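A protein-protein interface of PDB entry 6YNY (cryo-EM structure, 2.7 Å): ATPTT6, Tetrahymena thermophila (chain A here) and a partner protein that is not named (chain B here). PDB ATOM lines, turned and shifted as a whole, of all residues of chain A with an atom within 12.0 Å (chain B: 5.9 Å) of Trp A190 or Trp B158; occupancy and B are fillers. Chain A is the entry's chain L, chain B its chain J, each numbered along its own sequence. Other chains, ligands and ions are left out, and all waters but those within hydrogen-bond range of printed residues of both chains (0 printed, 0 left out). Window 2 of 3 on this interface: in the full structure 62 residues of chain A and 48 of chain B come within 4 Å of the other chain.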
ATOM      1  N   ASP A 166       2.057 -18.707 -23.860  1.00  0.00           N
ATOM      2  CA  ASP A 166       2.406 -20.118 -23.967  1.00  0.00           C
ATOM      3  C   ASP A 166       1.903 -20.735 -25.266  1.00  0.00           C
ATOM      4  O   ASP A 166       2.617 -21.520 -25.897  1.00  0.00           O
ATOM      5  CB  ASP A 166       1.844 -20.887 -22.772  1.00  0.00           C
ATOM      6  CG  ASP A 166       2.477 -20.476 -21.460  1.00  0.00           C
ATOM      7  OD1 ASP A 166       2.222 -19.345 -21.001  1.00  0.00           O
ATOM      8  OD2 ASP A 166       3.228 -21.288 -20.884  1.00  0.00           O
ATOM      9  N   ASN A 167       0.680 -20.399 -25.680  1.00  0.00           N
ATOM     10  CA  ASN A 167       0.129 -20.999 -26.891  1.00  0.00           C
ATOM     11  C   ASN A 167       0.943 -20.625 -28.122  1.00  0.00           C
ATOM     12  O   ASN A 167       0.989 -21.392 -29.088  1.00  0.00           O
ATOM     13  CB  ASN A 167      -1.328 -20.577 -27.079  1.00  0.00           C
ATOM     14  CG  ASN A 167      -2.227 -21.063 -25.966  1.00  0.00           C
ATOM     15  OD1 ASN A 167      -2.997 -20.296 -25.396  1.00  0.00           O
ATOM     16  ND2 ASN A 167      -2.134 -22.342 -25.650  1.00  0.00           N
ATOM     17  N   LYS A 170       3.801 -23.195 -28.319  1.00  0.00           N
ATOM     18  CA  LYS A 170       3.383 -24.520 -28.757  1.00  0.00           C
ATOM     19  C   LYS A 170       3.111 -24.549 -30.254  1.00  0.00           C
ATOM     20  O   LYS A 170       3.435 -25.529 -30.935  1.00  0.00           O
ATOM     21  CB  LYS A 170       2.138 -24.948 -27.985  1.00  0.00           C
ATOM     22  CG  LYS A 170       2.277 -24.880 -26.485  1.00  0.00           C
ATOM     23  CD  LYS A 170       0.950 -25.141 -25.811  1.00  0.00           C
ATOM     24  CE  LYS A 170       1.021 -24.895 -24.321  1.00  0.00           C
ATOM     25  NZ  LYS A 170       1.992 -25.796 -23.667  1.00  0.00           N
ATOM     26  N   ARG A 176       2.924 -32.093 -32.789  1.00  0.00           N
ATOM     27  CA  ARG A 176       2.521 -33.235 -31.989  1.00  0.00           C
ATOM     28  C   ARG A 176       2.134 -34.412 -32.870  1.00  0.00           C
ATOM     29  O   ARG A 176       1.636 -34.250 -33.986  1.00  0.00           O
ATOM     30  CB  ARG A 176       1.370 -32.855 -31.065  1.00  0.00           C
ATOM     31  CG  ARG A 176       1.802 -31.933 -29.955  1.00  0.00           C
ATOM     32  CD  ARG A 176       0.710 -31.687 -28.960  1.00  0.00           C
ATOM     33  NE  ARG A 176       1.243 -31.173 -27.704  1.00  0.00           N
ATOM     34  CZ  ARG A 176       1.673 -31.937 -26.707  1.00  0.00           C
ATOM     35  NH1 ARG A 176       1.636 -33.259 -26.807  1.00  0.00           N
ATOM     36  NH2 ARG A 176       2.146 -31.379 -25.605  1.00  0.00           N
ATOM     37  N   GLN A 181      -6.164 -43.031 -30.521  1.00  0.00           N
ATOM     38  CA  GLN A 181      -7.285 -42.236 -30.029  1.00  0.00           C
ATOM     39  C   GLN A 181      -7.078 -40.821 -30.550  1.00  0.00           C
ATOM     40  O   GLN A 181      -6.521 -39.945 -29.884  1.00  0.00           O
ATOM     41  CB  GLN A 181      -7.363 -42.281 -28.512  1.00  0.00           C
ATOM     42  CG  GLN A 181      -8.531 -41.521 -27.928  1.00  0.00           C
ATOM     43  CD  GLN A 181      -8.584 -41.610 -26.424  1.00  0.00           C
ATOM     44  OE1 GLN A 181      -8.519 -42.697 -25.852  1.00  0.00           O
ATOM     45  NE2 GLN A 181      -8.691 -40.465 -25.771  1.00  0.00           N
ATOM     46  N   ASN A 183      -7.250 -37.502 -30.984  1.00  0.00           N
ATOM     47  CA  ASN A 183      -7.845 -36.371 -30.296  1.00  0.00           C
ATOM     48  C   ASN A 183      -6.754 -35.388 -29.909  1.00  0.00           C
ATOM     49  O   ASN A 183      -5.585 -35.754 -29.763  1.00  0.00           O
ATOM     50  CB  ASN A 183      -8.608 -36.803 -29.041  1.00  0.00           C
ATOM     51  CG  ASN A 183      -9.967 -37.385 -29.352  1.00  0.00           C
ATOM     52  OD1 ASN A 183     -10.194 -38.583 -29.198  1.00  0.00           O
ATOM     53  ND2 ASN A 183     -10.889 -36.531 -29.779  1.00  0.00           N
ATOM     54  N   ILE A 184      -7.151 -34.135 -29.763  1.00  0.00           N
ATOM     55  CA  ILE A 184      -6.251 -33.122 -29.207  1.00  0.00           C
ATOM     56  C   ILE A 184      -6.006 -33.439 -27.738  1.00  0.00           C
ATOM     57  O   ILE A 184      -6.921 -33.939 -27.060  1.00  0.00           O
ATOM     58  CB  ILE A 184      -6.859 -31.729 -29.391  1.00  0.00           C
ATOM     59  CG1 ILE A 184      -6.928 -31.397 -30.878  1.00  0.00           C
ATOM     60  CG2 ILE A 184      -6.073 -30.674 -28.656  1.00  0.00           C
ATOM     61  CD1 ILE A 184      -7.835 -30.266 -31.206  1.00  0.00           C
ATOM     62  N   PRO A 185      -4.810 -33.198 -27.203  1.00  0.00           N
ATOM     63  CA  PRO A 185      -4.562 -33.520 -25.795  1.00  0.00           C
ATOM     64  C   PRO A 185      -5.598 -32.890 -24.879  1.00  0.00           C
ATOM     65  O   PRO A 185      -6.005 -31.741 -25.062  1.00  0.00           O
ATOM     66  CB  PRO A 185      -3.163 -32.954 -25.549  1.00  0.00           C
ATOM     67  CG  PRO A 185      -2.518 -33.006 -26.876  1.00  0.00           C
ATOM     68  CD  PRO A 185      -3.589 -32.719 -27.869  1.00  0.00           C
ATOM     69  N   GLU A 186      -6.027 -33.665 -23.883  1.00  0.00           N
ATOM     70  CA  GLU A 186      -7.051 -33.192 -22.959  1.00  0.00           C
ATOM     71  C   GLU A 186      -6.615 -31.916 -22.252  1.00  0.00           C
ATOM     72  O   GLU A 186      -7.426 -31.011 -22.037  1.00  0.00           O
ATOM     73  CB  GLU A 186      -7.373 -34.287 -21.946  1.00  0.00           C
ATOM     74  CG  GLU A 186      -8.353 -33.871 -20.880  1.00  0.00           C
ATOM     75  CD  GLU A 186      -8.860 -35.042 -20.077  1.00  0.00           C
ATOM     76  OE1 GLU A 186     -10.092 -35.216 -19.990  1.00  0.00           O
ATOM     77  OE2 GLU A 186      -8.025 -35.797 -19.537  1.00  0.00           O
ATOM     78  N   ALA A 187      -5.339 -31.828 -21.877  1.00  0.00           N
ATOM     79  CA  ALA A 187      -4.839 -30.610 -21.254  1.00  0.00           C
ATOM     80  C   ALA A 187      -4.983 -29.416 -22.186  1.00  0.00           C
ATOM     81  O   ALA A 187      -5.348 -28.319 -21.751  1.00  0.00           O
ATOM     82  CB  ALA A 187      -3.381 -30.791 -20.849  1.00  0.00           C
ATOM     83  N   THR A 188      -4.698 -29.612 -23.472  1.00  0.00           N
ATOM     84  CA  THR A 188      -4.831 -28.526 -24.434  1.00  0.00           C
ATOM     85  C   THR A 188      -6.291 -28.134 -24.621  1.00  0.00           C
ATOM     86  O   THR A 188      -6.605 -26.948 -24.768  1.00  0.00           O
ATOM     87  CB  THR A 188      -4.199 -28.940 -25.761  1.00  0.00           C
ATOM     88  OG1 THR A 188      -2.796 -29.151 -25.574  1.00  0.00           O
ATOM     89  CG2 THR A 188      -4.405 -27.887 -26.821  1.00  0.00           C
ATOM     90  N   ARG A 189      -7.194 -29.113 -24.616  1.00  0.00           N
ATOM     91  CA  ARG A 189      -8.616 -28.804 -24.715  1.00  0.00           C
ATOM     92  C   ARG A 189      -9.115 -28.093 -23.465  1.00  0.00           C
ATOM     93  O   ARG A 189      -9.932 -27.171 -23.553  1.00  0.00           O
ATOM     94  CB  ARG A 189      -9.417 -30.080 -24.954  1.00  0.00           C
ATOM     95  CG  ARG A 189      -9.317 -30.623 -26.360  1.00  0.00           C
ATOM     96  CD  ARG A 189      -9.177 -32.126 -26.371  1.00  0.00           C
ATOM     97  NE  ARG A 189     -10.409 -32.825 -26.038  1.00  0.00           N
ATOM     98  CZ  ARG A 189     -10.468 -34.125 -25.774  1.00  0.00           C
ATOM     99  NH1 ARG A 189      -9.365 -34.856 -25.793  1.00  0.00           N
ATOM    100  NH2 ARG A 189     -11.627 -34.693 -25.486  1.00  0.00           N
ATOM    101  N   TRP A 190      -8.634 -28.505 -22.293  1.00  0.00           N
ATOM    102  CA  TRP A 190      -9.093 -27.898 -21.051  1.00  0.00           C
ATOM    103  C   TRP A 190      -8.639 -26.450 -20.944  1.00  0.00           C
ATOM    104  O   TRP A 190      -9.428 -25.567 -20.592  1.00  0.00           O
ATOM    105  CB  TRP A 190      -8.593 -28.711 -19.862  1.00  0.00           C
ATOM    106  CG  TRP A 190      -9.103 -28.215 -18.563  1.00  0.00           C
ATOM    107  CD1 TRP A 190     -10.259 -28.571 -17.950  1.00  0.00           C
ATOM    108  CD2 TRP A 190      -8.475 -27.257 -17.712  1.00  0.00           C
ATOM    109  NE1 TRP A 190     -10.395 -27.899 -16.768  1.00  0.00           N
ATOM    110  CE2 TRP A 190      -9.310 -27.084 -16.598  1.00  0.00           C
ATOM    111  CE3 TRP A 190      -7.288 -26.531 -17.782  1.00  0.00           C
ATOM    112  CZ2 TRP A 190      -8.996 -26.214 -15.567  1.00  0.00           C
ATOM    113  CZ3 TRP A 190      -6.981 -25.673 -16.761  1.00  0.00           C
ATOM    114  CH2 TRP A 190      -7.828 -25.519 -15.666  1.00  0.00           C
ATOM    115  N   TYR A 191      -7.365 -26.187 -21.233  1.00  0.00           N
ATOM    116  CA  TYR A 191      -6.885 -24.813 -21.241  1.00  0.00           C
ATOM    117  C   TYR A 191      -7.656 -23.957 -22.233  1.00  0.00           C
ATOM    118  O   TYR A 191      -7.864 -22.764 -21.992  1.00  0.00           O
ATOM    119  CB  TYR A 191      -5.395 -24.771 -21.570  1.00  0.00           C
ATOM    120  CG  TYR A 191      -4.483 -25.067 -20.410  1.00  0.00           C
ATOM    121  CD1 TYR A 191      -4.409 -24.210 -19.329  1.00  0.00           C
ATOM    122  CD2 TYR A 191      -3.674 -26.190 -20.407  1.00  0.00           C
ATOM    123  CE1 TYR A 191      -3.576 -24.469 -18.274  1.00  0.00           C
ATOM    124  CE2 TYR A 191      -2.836 -26.456 -19.357  1.00  0.00           C
ATOM    125  CZ  TYR A 191      -2.788 -25.590 -18.292  1.00  0.00           C
ATOM    126  OH  TYR A 191      -1.952 -25.851 -17.238  1.00  0.00           O
ATOM    127  N   GLY A 192      -8.091 -24.545 -23.347  1.00  0.00           N
ATOM    128  CA  GLY A 192      -8.796 -23.798 -24.371  1.00  0.00           C
ATOM    129  C   GLY A 192     -10.202 -23.386 -23.999  1.00  0.00           C
ATOM    130  O   GLY A 192     -10.773 -22.517 -24.663  1.00  0.00           O
ATOM    131  N   ARG A 193     -10.777 -23.988 -22.961  1.00  0.00           N
ATOM    132  CA  ARG A 193     -12.123 -23.633 -22.538  1.00  0.00           C
ATOM    133  C   ARG A 193     -12.153 -22.503 -21.525  1.00  0.00           C
ATOM    134  O   ARG A 193     -13.206 -21.884 -21.345  1.00  0.00           O
ATOM    135  CB  ARG A 193     -12.828 -24.853 -21.952  1.00  0.00           C
ATOM    136  CG  ARG A 193     -12.974 -25.973 -22.931  1.00  0.00           C
ATOM    137  CD  ARG A 193     -13.838 -27.086 -22.391  1.00  0.00           C
ATOM    138  NE  ARG A 193     -13.417 -28.385 -22.906  1.00  0.00           N
ATOM    139  CZ  ARG A 193     -12.701 -29.274 -22.227  1.00  0.00           C
ATOM    140  NH1 ARG A 193     -12.369 -30.418 -22.797  1.00  0.00           N
ATOM    141  NH2 ARG A 193     -12.328 -29.038 -20.980  1.00  0.00           N
ATOM    142  N   GLN A 194     -11.039 -22.222 -20.864  1.00  0.00           N
ATOM    143  CA  GLN A 194     -10.981 -21.082 -19.964  1.00  0.00           C
ATOM    144  C   GLN A 194     -11.266 -19.837 -20.792  1.00  0.00           C
ATOM    145  O   GLN A 194     -10.422 -19.420 -21.594  1.00  0.00           O
ATOM    146  CB  GLN A 194      -9.625 -20.990 -19.274  1.00  0.00           C
ATOM    147  CG  GLN A 194      -9.170 -22.281 -18.630  1.00  0.00           C
ATOM    148  CD  GLN A 194     -10.185 -22.845 -17.664  1.00  0.00           C
ATOM    149  OE1 GLN A 194     -10.576 -22.192 -16.699  1.00  0.00           O
ATOM    150  NE2 GLN A 194     -10.627 -24.062 -17.925  1.00  0.00           N
ATOM    151  N   PRO A 195     -12.429 -19.214 -20.627  1.00  0.00           N
ATOM    152  CA  PRO A 195     -12.866 -18.217 -21.607  1.00  0.00           C
ATOM    153  C   PRO A 195     -12.010 -16.965 -21.587  1.00  0.00           C
ATOM    154  O   PRO A 195     -11.620 -16.464 -20.530  1.00  0.00           O
ATOM    155  CB  PRO A 195     -14.303 -17.919 -21.180  1.00  0.00           C
ATOM    156  CG  PRO A 195     -14.328 -18.210 -19.739  1.00  0.00           C
ATOM    157  CD  PRO A 195     -13.389 -19.345 -19.520  1.00  0.00           C
ATOM    158  N   GLY A 196     -11.719 -16.464 -22.782  1.00  0.00           N
ATOM    159  CA  GLY A 196     -11.051 -15.194 -22.917  1.00  0.00           C
ATOM    160  C   GLY A 196     -12.004 -14.032 -22.758  1.00  0.00           C
ATOM    161  O   GLY A 196     -13.219 -14.187 -22.666  1.00  0.00           O
ATOM    162  N   ASN A 227      -7.874 -11.583 -13.733  1.00  0.00           N
ATOM    163  CA  ASN A 227      -8.909 -12.228 -14.528  1.00  0.00           C
ATOM    164  C   ASN A 227     -10.281 -11.605 -14.292  1.00  0.00           C
ATOM    165  O   ASN A 227     -11.298 -12.250 -14.553  1.00  0.00           O
ATOM    166  CB  ASN A 227      -8.956 -13.720 -14.213  1.00  0.00           C
ATOM    167  CG  ASN A 227      -9.136 -13.995 -12.741  1.00  0.00           C
ATOM    168  OD1 ASN A 227      -9.429 -13.094 -11.960  1.00  0.00           O
ATOM    169  ND2 ASN A 227      -8.966 -15.245 -12.353  1.00  0.00           N
ATOM    170  N   ALA A 234     -15.488 -14.605 -24.248  1.00  0.00           N
ATOM    171  CA  ALA A 234     -15.480 -15.131 -25.610  1.00  0.00           C
ATOM    172  C   ALA A 234     -15.834 -16.617 -25.584  1.00  0.00           C
ATOM    173  O   ALA A 234     -15.017 -17.500 -25.850  1.00  0.00           O
ATOM    174  CB  ALA A 234     -14.130 -14.891 -26.266  1.00  0.00           C
ATOM    175  N   ASP A 235     -17.098 -16.883 -25.251  1.00  0.00           N
ATOM    176  CA  ASP A 235     -17.626 -18.231 -25.237  1.00  0.00           C
ATOM    177  C   ASP A 235     -18.993 -18.203 -25.914  1.00  0.00           C
ATOM    178  O   ASP A 235     -19.805 -17.309 -25.623  1.00  0.00           O
ATOM    179  CB  ASP A 235     -17.740 -18.775 -23.813  1.00  0.00           C
ATOM    180  CG  ASP A 235     -18.021 -20.263 -23.775  1.00  0.00           C
ATOM    181  OD1 ASP A 235     -17.054 -21.051 -23.749  1.00  0.00           O
ATOM    182  OD2 ASP A 235     -19.207 -20.648 -23.776  1.00  0.00           O
ATOM    183  N   GLU B 119       3.443 -30.877 -20.369  1.00  0.00           N
ATOM    184  CA  GLU B 119       2.523 -29.785 -20.110  1.00  0.00           C
ATOM    185  C   GLU B 119       2.730 -29.238 -18.707  1.00  0.00           C
ATOM    186  O   GLU B 119       3.163 -29.943 -17.792  1.00  0.00           O
ATOM    187  CB  GLU B 119       1.075 -30.239 -20.285  1.00  0.00           C
ATOM    188  CG  GLU B 119       0.659 -30.428 -21.731  1.00  0.00           C
ATOM    189  CD  GLU B 119       0.558 -29.113 -22.485  1.00  0.00           C
ATOM    190  OE1 GLU B 119       0.570 -28.049 -21.830  1.00  0.00           O
ATOM    191  OE2 GLU B 119       0.466 -29.143 -23.730  1.00  0.00           O
ATOM    192  N   LYS B 120       2.420 -27.960 -18.549  1.00  0.00           N
ATOM    193  CA  LYS B 120       2.533 -27.279 -17.271  1.00  0.00           C
ATOM    194  C   LYS B 120       1.193 -27.374 -16.554  1.00  0.00           C
ATOM    195  O   LYS B 120       0.173 -26.910 -17.073  1.00  0.00           O
ATOM    196  CB  LYS B 120       2.943 -25.825 -17.489  1.00  0.00           C
ATOM    197  CG  LYS B 120       3.543 -25.142 -16.289  1.00  0.00           C
ATOM    198  CD  LYS B 120       4.463 -24.016 -16.730  1.00  0.00           C
ATOM    199  CE  LYS B 120       3.713 -22.944 -17.505  1.00  0.00           C
ATOM    200  NZ  LYS B 120       4.629 -21.888 -18.012  1.00  0.00           N
ATOM    201  N   LEU B 121       1.193 -27.992 -15.375  1.00  0.00           N
ATOM    202  CA  LEU B 121      -0.047 -28.168 -14.646  1.00  0.00           C
ATOM    203  C   LEU B 121      -0.634 -26.811 -14.276  1.00  0.00           C
ATOM    204  O   LEU B 121       0.078 -25.806 -14.220  1.00  0.00           O
ATOM    205  CB  LEU B 121       0.175 -28.998 -13.387  1.00  0.00           C
ATOM    206  CG  LEU B 121       0.629 -30.443 -13.580  1.00  0.00           C
ATOM    207  CD1 LEU B 121       0.702 -31.141 -12.244  1.00  0.00           C
ATOM    208  CD2 LEU B 121      -0.297 -31.189 -14.510  1.00  0.00           C
ATOM    209  N   PRO B 122      -1.939 -26.757 -14.024  1.00  0.00           N
ATOM    210  CA  PRO B 122      -2.560 -25.481 -13.673  1.00  0.00           C
ATOM    211  C   PRO B 122      -1.944 -24.889 -12.418  1.00  0.00           C
ATOM    212  O   PRO B 122      -1.531 -25.600 -11.502  1.00  0.00           O
ATOM    213  CB  PRO B 122      -4.031 -25.847 -13.461  1.00  0.00           C
ATOM    214  CG  PRO B 122      -4.215 -27.111 -14.176  1.00  0.00           C
ATOM    215  CD  PRO B 122      -2.930 -27.840 -14.085  1.00  0.00           C
ATOM    216  N   PRO B 156      -7.756 -30.460 -11.813  1.00  0.00           N
ATOM    217  CA  PRO B 156      -8.632 -31.144 -12.763  1.00  0.00           C
ATOM    218  C   PRO B 156      -8.188 -32.579 -12.994  1.00  0.00           C
ATOM    219  O   PRO B 156      -7.026 -32.943 -12.802  1.00  0.00           O
ATOM    220  CB  PRO B 156      -8.516 -30.297 -14.034  1.00  0.00           C
ATOM    221  CG  PRO B 156      -7.292 -29.512 -13.870  1.00  0.00           C
ATOM    222  CD  PRO B 156      -7.118 -29.282 -12.419  1.00  0.00           C
ATOM    223  N   ASN B 157      -9.145 -33.404 -13.415  1.00  0.00           N
ATOM    224  CA  ASN B 157      -8.895 -34.835 -13.520  1.00  0.00           C
ATOM    225  C   ASN B 157      -7.797 -35.151 -14.525  1.00  0.00           C
ATOM    226  O   ASN B 157      -7.029 -36.096 -14.322  1.00  0.00           O
ATOM    227  CB  ASN B 157     -10.184 -35.564 -13.885  1.00  0.00           C
ATOM    228  CG  ASN B 157     -11.160 -35.615 -12.737  1.00  0.00           C
ATOM    229  OD1 ASN B 157     -10.774 -35.829 -11.589  1.00  0.00           O
ATOM    230  ND2 ASN B 157     -12.431 -35.412 -13.035  1.00  0.00           N
ATOM    231  N   TRP B 158      -7.703 -34.384 -15.611  1.00  0.00           N
ATOM    232  CA  TRP B 158      -6.637 -34.635 -16.571  1.00  0.00           C
ATOM    233  C   TRP B 158      -5.267 -34.465 -15.931  1.00  0.00           C
ATOM    234  O   TRP B 158      -4.295 -35.084 -16.374  1.00  0.00           O
ATOM    235  CB  TRP B 158      -6.782 -33.717 -17.786  1.00  0.00           C
ATOM    236  CG  TRP B 158      -6.434 -32.285 -17.551  1.00  0.00           C
ATOM    237  CD1 TRP B 158      -7.301 -31.262 -17.349  1.00  0.00           C
ATOM    238  CD2 TRP B 158      -5.122 -31.711 -17.510  1.00  0.00           C
ATOM    239  NE1 TRP B 158      -6.619 -30.087 -17.179  1.00  0.00           N
ATOM    240  CE2 TRP B 158      -5.277 -30.338 -17.269  1.00  0.00           C
ATOM    241  CE3 TRP B 158      -3.834 -32.228 -17.644  1.00  0.00           C
ATOM    242  CZ2 TRP B 158      -4.197 -29.477 -17.164  1.00  0.00           C
ATOM    243  CZ3 TRP B 158      -2.764 -31.370 -17.538  1.00  0.00           C
ATOM    244  CH2 TRP B 158      -2.950 -30.012 -17.301  1.00  0.00           C
ATOM    245  N   ALA B 159      -5.173 -33.643 -14.887  1.00  0.00           N
ATOM    246  CA  ALA B 159      -3.907 -33.476 -14.186  1.00  0.00           C
ATOM    247  C   ALA B 159      -3.636 -34.646 -13.252  1.00  0.00           C
ATOM    248  O   ALA B 159      -2.495 -35.104 -13.141  1.00  0.00           O
ATOM    249  CB  ALA B 159      -3.909 -32.162 -13.411  1.00  0.00           C
ATOM    250  N   LEU B 160      -4.672 -35.141 -12.574  1.00  0.00           N
ATOM    251  CA  LEU B 160      -4.503 -36.298 -11.704  1.00  0.00           C
ATOM    252  C   LEU B 160      -4.077 -37.526 -12.490  1.00  0.00           C
ATOM    253  O   LEU B 160      -3.319 -38.359 -11.981  1.00  0.00           O
ATOM    254  CB  LEU B 160      -5.798 -36.576 -10.950  1.00  0.00           C
ATOM    255  CG  LEU B 160      -6.358 -35.423 -10.121  1.00  0.00           C
ATOM    256  CD1 LEU B 160      -7.706 -35.787  -9.558  1.00  0.00           C
ATOM    257  CD2 LEU B 160      -5.414 -35.043  -9.007  1.00  0.00           C
ATOM    258  N   ASP B 161      -4.554 -37.662 -13.727  1.00  0.00           N
ATOM    259  CA  ASP B 161      -4.112 -38.761 -14.574  1.00  0.00           C
ATOM    260  C   ASP B 161      -2.639 -38.620 -14.936  1.00  0.00           C
ATOM    261  O   ASP B 161      -1.897 -39.608 -14.941  1.00  0.00           O
ATOM    262  CB  ASP B 161      -4.971 -38.822 -15.834  1.00  0.00           C
ATOM    263  CG  ASP B 161      -6.399 -39.236 -15.546  1.00  0.00           C
ATOM    264  OD1 ASP B 161      -6.706 -39.557 -14.379  1.00  0.00           O
ATOM    265  OD2 ASP B 161      -7.217 -39.242 -16.489  1.00  0.00           O
ATOM    266  N   HIS B 162      -2.199 -37.400 -15.247  1.00  0.00           N
ATOM    267  CA  HIS B 162      -0.783 -37.170 -15.509  1.00  0.00           C
ATOM    268  C   HIS B 162       0.059 -37.510 -14.290  1.00  0.00           C
ATOM    269  O   HIS B 162       1.079 -38.201 -14.396  1.00  0.00           O
ATOM    270  CB  HIS B 162      -0.555 -35.719 -15.923  1.00  0.00           C
ATOM    271  CG  HIS B 162      -0.944 -35.423 -17.336  1.00  0.00           C
ATOM    272  ND1 HIS B 162      -0.278 -34.499 -18.109  1.00  0.00           N
ATOM    273  CD2 HIS B 162      -1.930 -35.924 -18.115  1.00  0.00           C
ATOM    274  CE1 HIS B 162      -0.833 -34.447 -19.306  1.00  0.00           C
ATOM    275  NE2 HIS B 162      -1.838 -35.301 -19.334  1.00  0.00           N
ATOM    276  N   MET B 163      -0.352 -37.028 -13.117  1.00  0.00           N
ATOM    277  CA  MET B 163       0.375 -37.341 -11.894  1.00  0.00           C
ATOM    278  C   MET B 163       0.410 -38.842 -11.648  1.00  0.00           C
ATOM    279  O   MET B 163       1.431 -39.388 -11.219  1.00  0.00           O
ATOM    280  CB  MET B 163      -0.276 -36.617 -10.720  1.00  0.00           C
ATOM    281  CG  MET B 163      -0.288 -35.113 -10.873  1.00  0.00           C
ATOM    282  SD  MET B 163      -1.495 -34.275  -9.836  1.00  0.00           S
ATOM    283  CE  MET B 163      -0.737 -34.490  -8.238  1.00  0.00           C
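Among the printed residues, merely in contact across the chains: Glu A186 with Trp B158 (3.0 Å), Tyr A191 with Leu B121 (3.4 Å), Trp A190 with Trp B158 (3.4 Å), Ala A187 with Trp B158 (3.4 Å), Thr A188 with Glu B119 (3.7 Å) and Tyr A191 with Trp B158 (3.97 Å).
OE1 of Glu B119 is in salt-bridge range of NZ of Lys A170, at 3.2 Å. OE2 of Glu B119 is in salt-bridge range of NH2 of Arg A176, 3.4 Å away. The side-chain carboxylate (OD2) of Asp A166 is in salt-bridge range of the side-chain amino group (NZ) of Lys B120, at 3.3 Å. OH of Tyr A191 sits close to O of Lys B120, 2.4 Å away. OH of Tyr A191 lies close to N of Pro B122, 3.3 Å away.
O of Trp A190 sits at hydrogen-bond distance from NE2 of Gln A194 (3.3 Å).
Trp A190 touches just one residue of chain B: Trp B158 (3.4 Å). Of chain A, only Glu A186, Ala A187, Trp A190 and Tyr A191 come within 4 Å of Trp B158. Of chain A, only Lys A170, Arg A176 and Thr A188 come within 4 Å of Glu B119. Of chain A, only Tyr A191 (3.3 Å) comes within 4 Å of Pro B122. No residue of chain A comes within 4 Å of Pro B156. No residue of chain A comes within 4 Å of Asn B157. No residue of chain A comes within 4 Å of Ala B159. No residue of chain A comes within 4 Å of Leu B160. No residue of chain A comes within 4 Å of Asp B161. No residue of chain A comes within 4 Å of His B162. Of the printed residues of chain B, Lys A170 touches Glu B119 (3.2 Å). Of the printed residues of chain B, Thr A188 touches Glu B119 (3.7 Å). The nearest residue of chain B that does not touch Trp A190 is Pro B122 (4.05 Å). The nearest residue of chain A that does not touch Trp B158 is Thr A188 (6.3 Å).
Of the 12 printed residues of chain B, 5 touch a printed residue of chain A. Along chain B the printed residues that touch a printed residue of chain A span positions 119 to 158. Printed residues of chain A that touch a printed residue of chain B: Asp A166, Lys A170, Arg A176, Glu A186, Ala A187, Thr A188, Trp A190 and Tyr A191. Hydrophobic or aromatic side chains of chain A that line the printed part of chain B: Ala A187, Trp A190 and Tyr A191. Among the printed residues, 11 pairs touch across the chains. Among the printed residues, Asp or Glu carboxylates within 4 Å of a Lys or Arg side-chain nitrogen of the other chain: Asp A166 with Lys B120 (3.3 Å), Lys A170 with Glu B119 (3.2 Å) and Arg A176 with Glu B119 (3.4 Å).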
